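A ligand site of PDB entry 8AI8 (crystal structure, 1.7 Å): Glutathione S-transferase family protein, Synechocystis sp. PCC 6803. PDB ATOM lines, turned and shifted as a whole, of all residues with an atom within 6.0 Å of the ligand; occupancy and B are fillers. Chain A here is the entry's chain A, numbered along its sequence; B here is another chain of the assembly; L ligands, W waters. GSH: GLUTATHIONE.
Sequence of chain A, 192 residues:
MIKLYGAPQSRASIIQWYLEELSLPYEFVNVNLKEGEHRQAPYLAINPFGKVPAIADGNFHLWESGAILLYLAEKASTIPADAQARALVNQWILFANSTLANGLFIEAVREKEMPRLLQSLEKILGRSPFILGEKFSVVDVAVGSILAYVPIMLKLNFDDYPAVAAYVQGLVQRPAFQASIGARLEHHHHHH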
ATOM      1  N   ALA A   7     -29.315  15.643  19.338  1.00  0.00           N
ATOM      2  CA  ALA A   7     -28.509  14.714  18.553  1.00  0.00           C
ATOM      3  C   ALA A   7     -28.333  13.424  19.363  1.00  0.00           C
ATOM      4  O   ALA A   7     -28.455  13.463  20.598  1.00  0.00           O
ATOM      5  CB  ALA A   7     -27.151  15.320  18.232  1.00  0.00           C
ATOM      6  N   GLN A   9     -27.210  10.544  21.739  1.00  0.00           N
ATOM      7  CA  GLN A   9     -26.331  10.486  22.922  1.00  0.00           C
ATOM      8  C   GLN A   9     -25.836  11.859  23.340  1.00  0.00           C
ATOM      9  O   GLN A   9     -24.655  12.022  23.653  1.00  0.00           O
ATOM     10  CB  GLN A   9     -25.139   9.517  22.674  1.00  0.00           C
ATOM     11  CG  GLN A   9     -25.538   8.168  22.083  1.00  0.00           C
ATOM     12  CD  GLN A   9     -26.483   7.417  22.988  1.00  0.00           C
ATOM     13  OE1 GLN A   9     -26.270   7.303  24.201  1.00  0.00           O
ATOM     14  NE2 GLN A   9     -27.540   6.873  22.401  1.00  0.00           N
ATOM     15  N   SER A  10     -26.731  12.866  23.337  1.00  0.00           N
ATOM     16  CA  SER A  10     -26.336  14.222  23.718  1.00  0.00           C
ATOM     17  C   SER A  10     -27.220  14.769  24.857  1.00  0.00           C
ATOM     18  O   SER A  10     -28.231  14.152  25.225  1.00  0.00           O
ATOM     19  CB  SER A  10     -26.362  15.152  22.495  1.00  0.00           C
ATOM     20  OG  SER A  10     -27.668  15.658  22.242  1.00  0.00           O
ATOM     21  N   ARG A  11     -26.883  15.955  25.367  1.00  0.00           N
ATOM     22  CA  ARG A  11     -27.641  16.597  26.436  1.00  0.00           C
ATOM     23  C   ARG A  11     -29.039  17.010  26.087  1.00  0.00           C
ATOM     24  O   ARG A  11     -29.782  17.428  26.986  1.00  0.00           O
ATOM     25  CB  ARG A  11     -26.886  17.803  26.982  1.00  0.00           C
ATOM     26  CG  ARG A  11     -25.616  17.355  27.635  1.00  0.00           C
ATOM     27  CD  ARG A  11     -24.862  18.513  28.207  1.00  0.00           C
ATOM     28  NE  ARG A  11     -23.927  18.040  29.215  1.00  0.00           N
ATOM     29  CZ  ARG A  11     -22.864  18.718  29.621  1.00  0.00           C
ATOM     30  NH1 ARG A  11     -22.576  19.904  29.103  1.00  0.00           N
ATOM     31  NH2 ARG A  11     -22.052  18.206  30.544  1.00  0.00           N
ATOM     32  N   LEU A  33     -24.680  15.976  13.919  1.00  0.00           N
ATOM     33  CA  LEU A  33     -23.341  16.451  14.321  1.00  0.00           C
ATOM     34  C   LEU A  33     -22.252  15.736  13.548  1.00  0.00           C
ATOM     35  O   LEU A  33     -21.260  16.364  13.146  1.00  0.00           O
ATOM     36  CB  LEU A  33     -23.109  16.225  15.831  1.00  0.00           C
ATOM     37  CG  LEU A  33     -24.110  16.861  16.801  1.00  0.00           C
ATOM     38  CD1 LEU A  33     -23.669  16.672  18.256  1.00  0.00           C
ATOM     39  CD2 LEU A  33     -24.343  18.328  16.498  1.00  0.00           C
ATOM     40  N   HIS A  38     -24.528  21.131  12.621  1.00  0.00           N
ATOM     41  CA  HIS A  38     -24.497  22.151  13.675  1.00  0.00           C
ATOM     42  C   HIS A  38     -23.605  23.345  13.312  1.00  0.00           C
ATOM     43  O   HIS A  38     -23.700  24.397  13.973  1.00  0.00           O
ATOM     44  CB  HIS A  38     -24.041  21.530  14.992  1.00  0.00           C
ATOM     45  CG  HIS A  38     -22.701  20.872  14.942  1.00  0.00           C
ATOM     46  ND1 HIS A  38     -22.411  19.867  14.003  1.00  0.00           N
ATOM     47  CD2 HIS A  38     -21.601  21.086  15.706  1.00  0.00           C
ATOM     48  CE1 HIS A  38     -21.152  19.502  14.250  1.00  0.00           C
ATOM     49  NE2 HIS A  38     -20.629  20.215  15.261  1.00  0.00           N
ATOM     50  N   ARG A  39     -22.708  23.185  12.313  1.00  0.00           N
ATOM     51  CA  ARG A  39     -21.798  24.256  11.853  1.00  0.00           C
ATOM     52  C   ARG A  39     -22.310  24.947  10.580  1.00  0.00           C
ATOM     53  O   ARG A  39     -21.569  25.741   9.996  1.00  0.00           O
ATOM     54  CB  ARG A  39     -20.371  23.729  11.623  1.00  0.00           C
ATOM     55  CG  ARG A  39     -19.817  22.885  12.763  1.00  0.00           C
ATOM     56  CD  ARG A  39     -19.462  23.685  14.000  1.00  0.00           C
ATOM     57  NE  ARG A  39     -18.562  24.810  13.703  1.00  0.00           N
ATOM     58  CZ  ARG A  39     -18.400  25.881  14.494  1.00  0.00           C
ATOM     59  NH1 ARG A  39     -19.051  25.960  15.649  1.00  0.00           N
ATOM     60  NH2 ARG A  39     -17.575  26.856  14.138  1.00  0.00           N
ATOM     61  N   PHE A  49     -22.731  29.253  18.644  1.00  0.00           N
ATOM     62  CA  PHE A  49     -21.632  28.399  19.068  1.00  0.00           C
ATOM     63  C   PHE A  49     -21.750  26.966  18.543  1.00  0.00           C
ATOM     64  O   PHE A  49     -20.874  26.159  18.827  1.00  0.00           O
ATOM     65  CB  PHE A  49     -21.474  28.445  20.603  1.00  0.00           C
ATOM     66  CG  PHE A  49     -21.163  29.855  21.024  1.00  0.00           C
ATOM     67  CD1 PHE A  49     -19.900  30.399  20.794  1.00  0.00           C
ATOM     68  CD2 PHE A  49     -22.148  30.696  21.509  1.00  0.00           C
ATOM     69  CE1 PHE A  49     -19.618  31.724  21.129  1.00  0.00           C
ATOM     70  CE2 PHE A  49     -21.874  32.029  21.822  1.00  0.00           C
ATOM     71  CZ  PHE A  49     -20.617  32.535  21.609  1.00  0.00           C
ATOM     72  N   GLY A  50     -22.813  26.658  17.798  1.00  0.00           N
ATOM     73  CA  GLY A  50     -23.007  25.355  17.165  1.00  0.00           C
ATOM     74  C   GLY A  50     -23.071  24.180  18.124  1.00  0.00           C
ATOM     75  O   GLY A  50     -22.475  23.131  17.863  1.00  0.00           O
ATOM     76  N   LYS A  51     -23.768  24.358  19.246  1.00  0.00           N
ATOM     77  CA  LYS A  51     -23.935  23.279  20.209  1.00  0.00           C
ATOM     78  C   LYS A  51     -25.402  22.944  20.400  1.00  0.00           C
ATOM     79  O   LYS A  51     -26.261  23.830  20.340  1.00  0.00           O
ATOM     80  CB  LYS A  51     -23.368  23.668  21.589  1.00  0.00           C
ATOM     81  CG  LYS A  51     -21.953  24.232  21.569  1.00  0.00           C
ATOM     82  CD  LYS A  51     -20.948  23.140  21.518  1.00  0.00           C
ATOM     83  CE  LYS A  51     -19.538  23.657  21.735  1.00  0.00           C
ATOM     84  NZ  LYS A  51     -18.584  22.535  21.802  1.00  0.00           N
ATOM     85  N   VAL A  52     -25.693  21.653  20.643  1.00  0.00           N
ATOM     86  CA  VAL A  52     -27.007  21.178  21.027  1.00  0.00           C
ATOM     87  C   VAL A  52     -26.936  20.839  22.545  1.00  0.00           C
ATOM     88  O   VAL A  52     -25.873  20.454  23.059  1.00  0.00           O
ATOM     89  CB  VAL A  52     -27.511  19.979  20.183  1.00  0.00           C
ATOM     90  CG1 VAL A  52     -27.780  20.411  18.740  1.00  0.00           C
ATOM     91  CG2 VAL A  52     -26.510  18.819  20.238  1.00  0.00           C
ATOM     92  N   PRO A  53     -28.026  21.011  23.278  1.00  0.00           N
ATOM     93  CA  PRO A  53     -29.368  21.374  22.782  1.00  0.00           C
ATOM     94  C   PRO A  53     -29.644  22.860  22.628  1.00  0.00           C
ATOM     95  O   PRO A  53     -28.910  23.723  23.115  1.00  0.00           O
ATOM     96  CB  PRO A  53     -30.276  20.800  23.877  1.00  0.00           C
ATOM     97  CG  PRO A  53     -29.457  21.082  25.148  1.00  0.00           C
ATOM     98  CD  PRO A  53     -28.058  20.682  24.723  1.00  0.00           C
ATOM     99  N   TRP A  63     -30.409  28.627  23.975  1.00  0.00           N
ATOM    100  CA  TRP A  63     -29.421  27.541  24.032  1.00  0.00           C
ATOM    101  C   TRP A  63     -28.788  27.515  25.474  1.00  0.00           C
ATOM    102  O   TRP A  63     -29.127  28.369  26.318  1.00  0.00           O
ATOM    103  CB  TRP A  63     -28.410  27.571  22.862  1.00  0.00           C
ATOM    104  CG  TRP A  63     -27.858  28.925  22.567  1.00  0.00           C
ATOM    105  CD1 TRP A  63     -28.423  29.887  21.769  1.00  0.00           C
ATOM    106  CD2 TRP A  63     -26.714  29.517  23.166  1.00  0.00           C
ATOM    107  NE1 TRP A  63     -27.668  31.030  21.812  1.00  0.00           N
ATOM    108  CE2 TRP A  63     -26.608  30.830  22.651  1.00  0.00           C
ATOM    109  CE3 TRP A  63     -25.727  29.049  24.047  1.00  0.00           C
ATOM    110  CZ2 TRP A  63     -25.590  31.709  23.053  1.00  0.00           C
ATOM    111  CZ3 TRP A  63     -24.708  29.914  24.422  1.00  0.00           C
ATOM    112  CH2 TRP A  63     -24.638  31.218  23.926  1.00  0.00           C
ATOM    113  N   GLU A  64     -27.976  26.479  25.730  1.00  0.00           N
ATOM    114  CA  GLU A  64     -27.383  26.036  27.001  1.00  0.00           C
ATOM    115  C   GLU A  64     -28.434  25.197  27.706  1.00  0.00           C
ATOM    116  O   GLU A  64     -29.485  25.707  28.112  1.00  0.00           O
ATOM    117  CB  GLU A  64     -26.902  27.178  27.917  1.00  0.00           C
ATOM    118  CG  GLU A  64     -25.568  27.750  27.475  1.00  0.00           C
ATOM    119  CD  GLU A  64     -24.408  26.778  27.506  1.00  0.00           C
ATOM    120  OE1 GLU A  64     -24.351  25.912  28.407  1.00  0.00           O
ATOM    121  OE2 GLU A  64     -23.523  26.906  26.624  1.00  0.00           O
ATOM    122  N   SER A  65     -28.154  23.905  27.868  1.00  0.00           N
ATOM    123  CA  SER A  65     -29.075  22.987  28.528  1.00  0.00           C
ATOM    124  C   SER A  65     -29.571  23.500  29.895  1.00  0.00           C
ATOM    125  O   SER A  65     -30.759  23.444  30.166  1.00  0.00           O
ATOM    126  CB  SER A  65     -28.452  21.595  28.667  1.00  0.00           C
ATOM    127  OG  SER A  65     -27.348  21.586  29.571  1.00  0.00           O
ATOM    128  N   GLY A  66     -28.664  24.108  30.672  1.00  0.00           N
ATOM    129  CA  GLY A  66     -29.052  24.636  31.978  1.00  0.00           C
ATOM    130  C   GLY A  66     -30.042  25.766  31.881  1.00  0.00           C
ATOM    131  O   GLY A  66     -31.001  25.828  32.657  1.00  0.00           O
ATOM    132  N   ASN A  97     -23.718  21.957  35.745  1.00  0.00           N
ATOM    133  CA  ASN A  97     -23.044  22.289  34.497  1.00  0.00           C
ATOM    134  C   ASN A  97     -21.578  22.666  34.612  1.00  0.00           C
ATOM    135  O   ASN A  97     -20.902  22.754  33.584  1.00  0.00           O
ATOM    136  CB  ASN A  97     -23.817  23.391  33.767  1.00  0.00           C
ATOM    137  CG  ASN A  97     -25.022  22.811  33.076  1.00  0.00           C
ATOM    138  OD1 ASN A  97     -24.921  22.303  31.946  1.00  0.00           O
ATOM    139  ND2 ASN A  97     -26.170  22.822  33.741  1.00  0.00           N
ATOM    140  N   LEU B  94     -24.599  30.584  31.867  1.00  0.00           N
ATOM    141  CA  LEU B  94     -24.315  29.149  31.753  1.00  0.00           C
ATOM    142  C   LEU B  94     -23.166  28.950  30.750  1.00  0.00           C
ATOM    143  O   LEU B  94     -22.247  28.176  31.016  1.00  0.00           O
ATOM    144  CB  LEU B  94     -25.562  28.349  31.311  1.00  0.00           C
ATOM    145  CG  LEU B  94     -26.375  27.656  32.423  1.00  0.00           C
ATOM    146  CD1 LEU B  94     -25.505  26.641  33.205  1.00  0.00           C
ATOM    147  CD2 LEU B  94     -27.026  28.655  33.338  1.00  0.00           C
ATOM    148  N   SER B  98     -19.512  27.191  31.558  1.00  0.00           N
ATOM    149  CA  SER B  98     -19.330  25.828  31.073  1.00  0.00           C
ATOM    150  C   SER B  98     -18.684  25.829  29.691  1.00  0.00           C
ATOM    151  O   SER B  98     -17.447  25.781  29.596  1.00  0.00           O
ATOM    152  CB  SER B  98     -20.666  25.056  31.104  1.00  0.00           C
ATOM    153  OG  SER B  98     -21.653  25.598  30.228  1.00  0.00           O
ATOM    154  N   THR B  99     -19.481  26.013  28.637  1.00  0.00           N
ATOM    155  CA  THR B  99     -18.995  25.975  27.247  1.00  0.00           C
ATOM    156  C   THR B  99     -17.750  26.822  27.005  1.00  0.00           C
ATOM    157  O   THR B  99     -16.752  26.336  26.458  1.00  0.00           O
ATOM    158  CB  THR B  99     -20.149  26.371  26.320  1.00  0.00           C
ATOM    159  OG1 THR B  99     -21.298  25.577  26.667  1.00  0.00           O
ATOM    160  CG2 THR B  99     -19.799  26.177  24.851  1.00  0.00           C
ATOM    161  N   LYS B 112      -9.110  22.593  19.544  1.00  0.00           N
ATOM    162  CA  LYS B 112     -10.293  22.572  18.705  1.00  0.00           C
ATOM    163  C   LYS B 112     -11.301  23.671  19.092  1.00  0.00           C
ATOM    164  O   LYS B 112     -11.793  24.406  18.230  1.00  0.00           O
ATOM    165  CB  LYS B 112     -10.957  21.185  18.731  1.00  0.00           C
ATOM    166  CG  LYS B 112     -12.216  21.113  17.872  1.00  0.00           C
ATOM    167  CD  LYS B 112     -12.962  19.805  18.058  1.00  0.00           C
ATOM    168  CE  LYS B 112     -14.090  19.675  17.073  1.00  0.00           C
ATOM    169  NZ  LYS B 112     -14.794  18.371  17.217  1.00  0.00           N
ATOM    170  N   GLU B 113     -11.639  23.755  20.389  1.00  0.00           N
ATOM    171  CA  GLU B 113     -12.692  24.640  20.882  1.00  0.00           C
ATOM    172  C   GLU B 113     -12.373  26.123  20.931  1.00  0.00           C
ATOM    173  O   GLU B 113     -13.231  26.924  20.561  1.00  0.00           O
ATOM    174  CB  GLU B 113     -13.144  24.200  22.290  1.00  0.00           C
ATOM    175  CG  GLU B 113     -13.673  22.780  22.333  1.00  0.00           C
ATOM    176  CD  GLU B 113     -15.018  22.637  21.654  1.00  0.00           C
ATOM    177  OE1 GLU B 113     -15.956  23.389  21.998  1.00  0.00           O
ATOM    178  OE2 GLU B 113     -15.127  21.760  20.753  1.00  0.00           O
ATOM    179  N   ARG B 116     -12.873  28.219  17.680  1.00  0.00           N
ATOM    180  CA  ARG B 116     -14.289  28.263  17.284  1.00  0.00           C
ATOM    181  C   ARG B 116     -15.073  29.239  18.172  1.00  0.00           C
ATOM    182  O   ARG B 116     -15.863  30.031  17.674  1.00  0.00           O
ATOM    183  CB  ARG B 116     -14.908  26.878  17.358  1.00  0.00           C
ATOM    184  CG  ARG B 116     -14.409  25.944  16.243  1.00  0.00           C
ATOM    185  CD  ARG B 116     -15.029  24.568  16.420  1.00  0.00           C
ATOM    186  NE  ARG B 116     -14.890  23.754  15.207  1.00  0.00           N
ATOM    187  CZ  ARG B 116     -15.606  22.663  14.961  1.00  0.00           C
ATOM    188  NH1 ARG B 116     -16.506  22.224  15.843  1.00  0.00           N
ATOM    189  NH2 ARG B 116     -15.426  21.990  13.826  1.00  0.00           N
HETATM  190  N1  GSH L   1     -22.774  23.667  28.215  1.00  0.00           N
HETATM  191  CA1 GSH L   1     -23.491  23.212  26.987  1.00  0.00           C
HETATM  192  C1  GSH L   1     -24.867  22.685  27.399  1.00  0.00           C
HETATM  193  O11 GSH L   1     -25.808  22.848  26.583  1.00  0.00           O
HETATM  194  O12 GSH L   1     -24.963  22.172  28.522  1.00  0.00           O
HETATM  195  CB1 GSH L   1     -22.687  22.115  26.293  1.00  0.00           C
HETATM  196  CG1 GSH L   1     -23.347  21.636  25.018  1.00  0.00           C
HETATM  197  CD1 GSH L   1     -22.503  20.630  24.249  1.00  0.00           C
HETATM  198  OE1 GSH L   1     -21.317  20.450  24.511  1.00  0.00           O
HETATM  199  N2  GSH L   1     -23.131  19.978  23.274  1.00  0.00           N
HETATM  200  CA2 GSH L   1     -22.447  19.040  22.403  1.00  0.00           C
HETATM  201  C2  GSH L   1     -22.290  19.577  20.975  1.00  0.00           C
HETATM  202  O2  GSH L   1     -23.258  20.093  20.429  1.00  0.00           O
HETATM  203  CB2 GSH L   1     -23.196  17.714  22.348  1.00  0.00           C
HETATM  204  SG2 GSH L   1     -22.298  16.435  21.447  1.00  0.00           S
HETATM  205  N3  GSH L   1     -21.102  19.427  20.392  1.00  0.00           N
HETATM  206  CA3 GSH L   1     -20.869  19.850  19.022  1.00  0.00           C
HETATM  207  C3  GSH L   1     -19.508  20.511  18.845  1.00  0.00           C
HETATM  208  O31 GSH L   1     -19.125  20.761  17.677  1.00  0.00           O
HETATM  209  O32 GSH L   1     -18.864  20.781  19.880  1.00  0.00           O
HETATM  210  O   HOH W   1     -19.745  22.571  28.204  1.00  0.00           O
HETATM  211  O   HOH W   2     -16.978  22.747  18.624  1.00  0.00           O
HETATM  212  O   HOH W   3     -18.392  20.266  23.713  1.00  0.00           O
HETATM  213  O   HOH W   4     -18.883  18.307  21.938  1.00  0.00           O
HETATM  214  O   HOH W   5     -20.056  19.706  27.008  1.00  0.00           O
HETATM  215  O   HOH W   6     -19.715  23.779  17.420  1.00  0.00           O
HETATM  216  O   HOH W   7     -22.481  22.094  30.667  1.00  0.00           O
HETATM  217  O   HOH W   8     -18.993  22.428  25.286  1.00  0.00           O
HETATM  218  O   HOH W   9     -25.858  24.636  30.364  1.00  0.00           O
HETATM  219  O   HOH W  10     -26.449  24.275  24.291  1.00  0.00           O
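Water W10 lies within hydrogen-bond range of an oxygen (O11) of the ligand (2.8 Å), the backbone carbonyl oxygen (O) of Pro 53 (2.8 Å) and the backbone NH (N) of Glu 64 (3.0 Å). Water W5 bridges an oxygen (OE1) of the ligand (2.9 Å) and the guanidinium group (NH1) of Arg 11 (3.3 Å). Water W7 lies within hydrogen-bond range of the guanidinium group of Arg 11 (2.7 Å), the side-chain amide oxygen of Asn 97 (2.8 Å) and a nitrogen (N1) of the ligand (2.9 Å). Water W3 bridges NZ of Lys 51 (3.0 Å) and OE1 of the ligand (3.0 Å). Water W9 lies within hydrogen-bond range of the side-chain carboxylate (OE1) of Glu 64 (2.8 Å), the backbone NH (N) of Gly 66 (2.9 Å), the side-chain amide oxygen (OD1) of Asn 97 (3.0 Å), an oxygen (O12) of the ligand (3.2 Å) and the backbone NH (N) of Ser 65 (3.5 Å). Water W1 bridges a nitrogen (N1) of the ligand (3.2 Å) and the backbone NH of Thr 99 of chain B (3.5 Å).
Leu 33 touches the ligand (CD1 to SG2, 3.5 Å). Gly 50 touches the ligand (O to CA3, 3.8 Å). CD of Pro 53 touches O11 of the ligand (3.6 Å). Glu 113 of chain B touches the ligand (OE2 to O32, 3.96 Å). Of the 23 residues printed, 14 come within 4 Å of the ligand. The nearest printed residue that does not touch the ligand is Ser 10 (4.1 Å).
The guanidinium group (NH1) of Arg 116 of chain B lies within salt-bridge range of an oxygen (O31) of the ligand (3.5 Å). The side-chain hydroxyl (OG1) of Thr 99 of chain B is in hydrogen-bond range of a nitrogen (N1) of the ligand. OD1 of Asn 97 sits close to O12 of the ligand. NE2 of His 38 is in hydrogen-bond range of O31 of the ligand (2.9 Å). A nitrogen (N1) of the ligand is in salt-bridge range of the side-chain carboxylate (OE1) of Glu 64. O of Val 52 lies within hydrogen-bond range of N2 of the ligand, at 2.8 Å. The guanidinium group (NH1) of Arg 11 lies within salt-bridge range of an oxygen (O12) of the ligand (3.3 Å). N1 of the ligand lies within hydrogen-bond range of OG of Ser 98 of chain B (3.0 Å). N of Val 52 lies within hydrogen-bond range of O2 of the ligand (2.9 Å). An oxygen (O11) of the ligand is in hydrogen-bond range of the backbone NH of Ser 65, 2.9 Å away. An oxygen (O12) of the ligand lies within hydrogen-bond range of the side-chain hydroxyl (OG) of Ser 65 (2.7 Å). The side-chain amino group (NZ) of Lys 51 is in salt-bridge range of an oxygen (O32) of the ligand (2.6 Å).
OE1 of Glu 64 sits at hydrogen-bond distance from OG of Ser 98 of chain B. OG of Ser 98 of chain B lies within hydrogen-bond range of O of Leu 94 of chain B. The side-chain carboxylate of Glu 64 is in hydrogen-bond range of the side-chain hydroxyl of Thr 99 of chain B (2.6 Å). NZ of Lys 51 is in salt-bridge range of OE1 of Glu 113 of chain B (2.8 Å). OG of Ser 65 lies within hydrogen-bond range of OD1 of Asn 97, at 3.5 Å.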
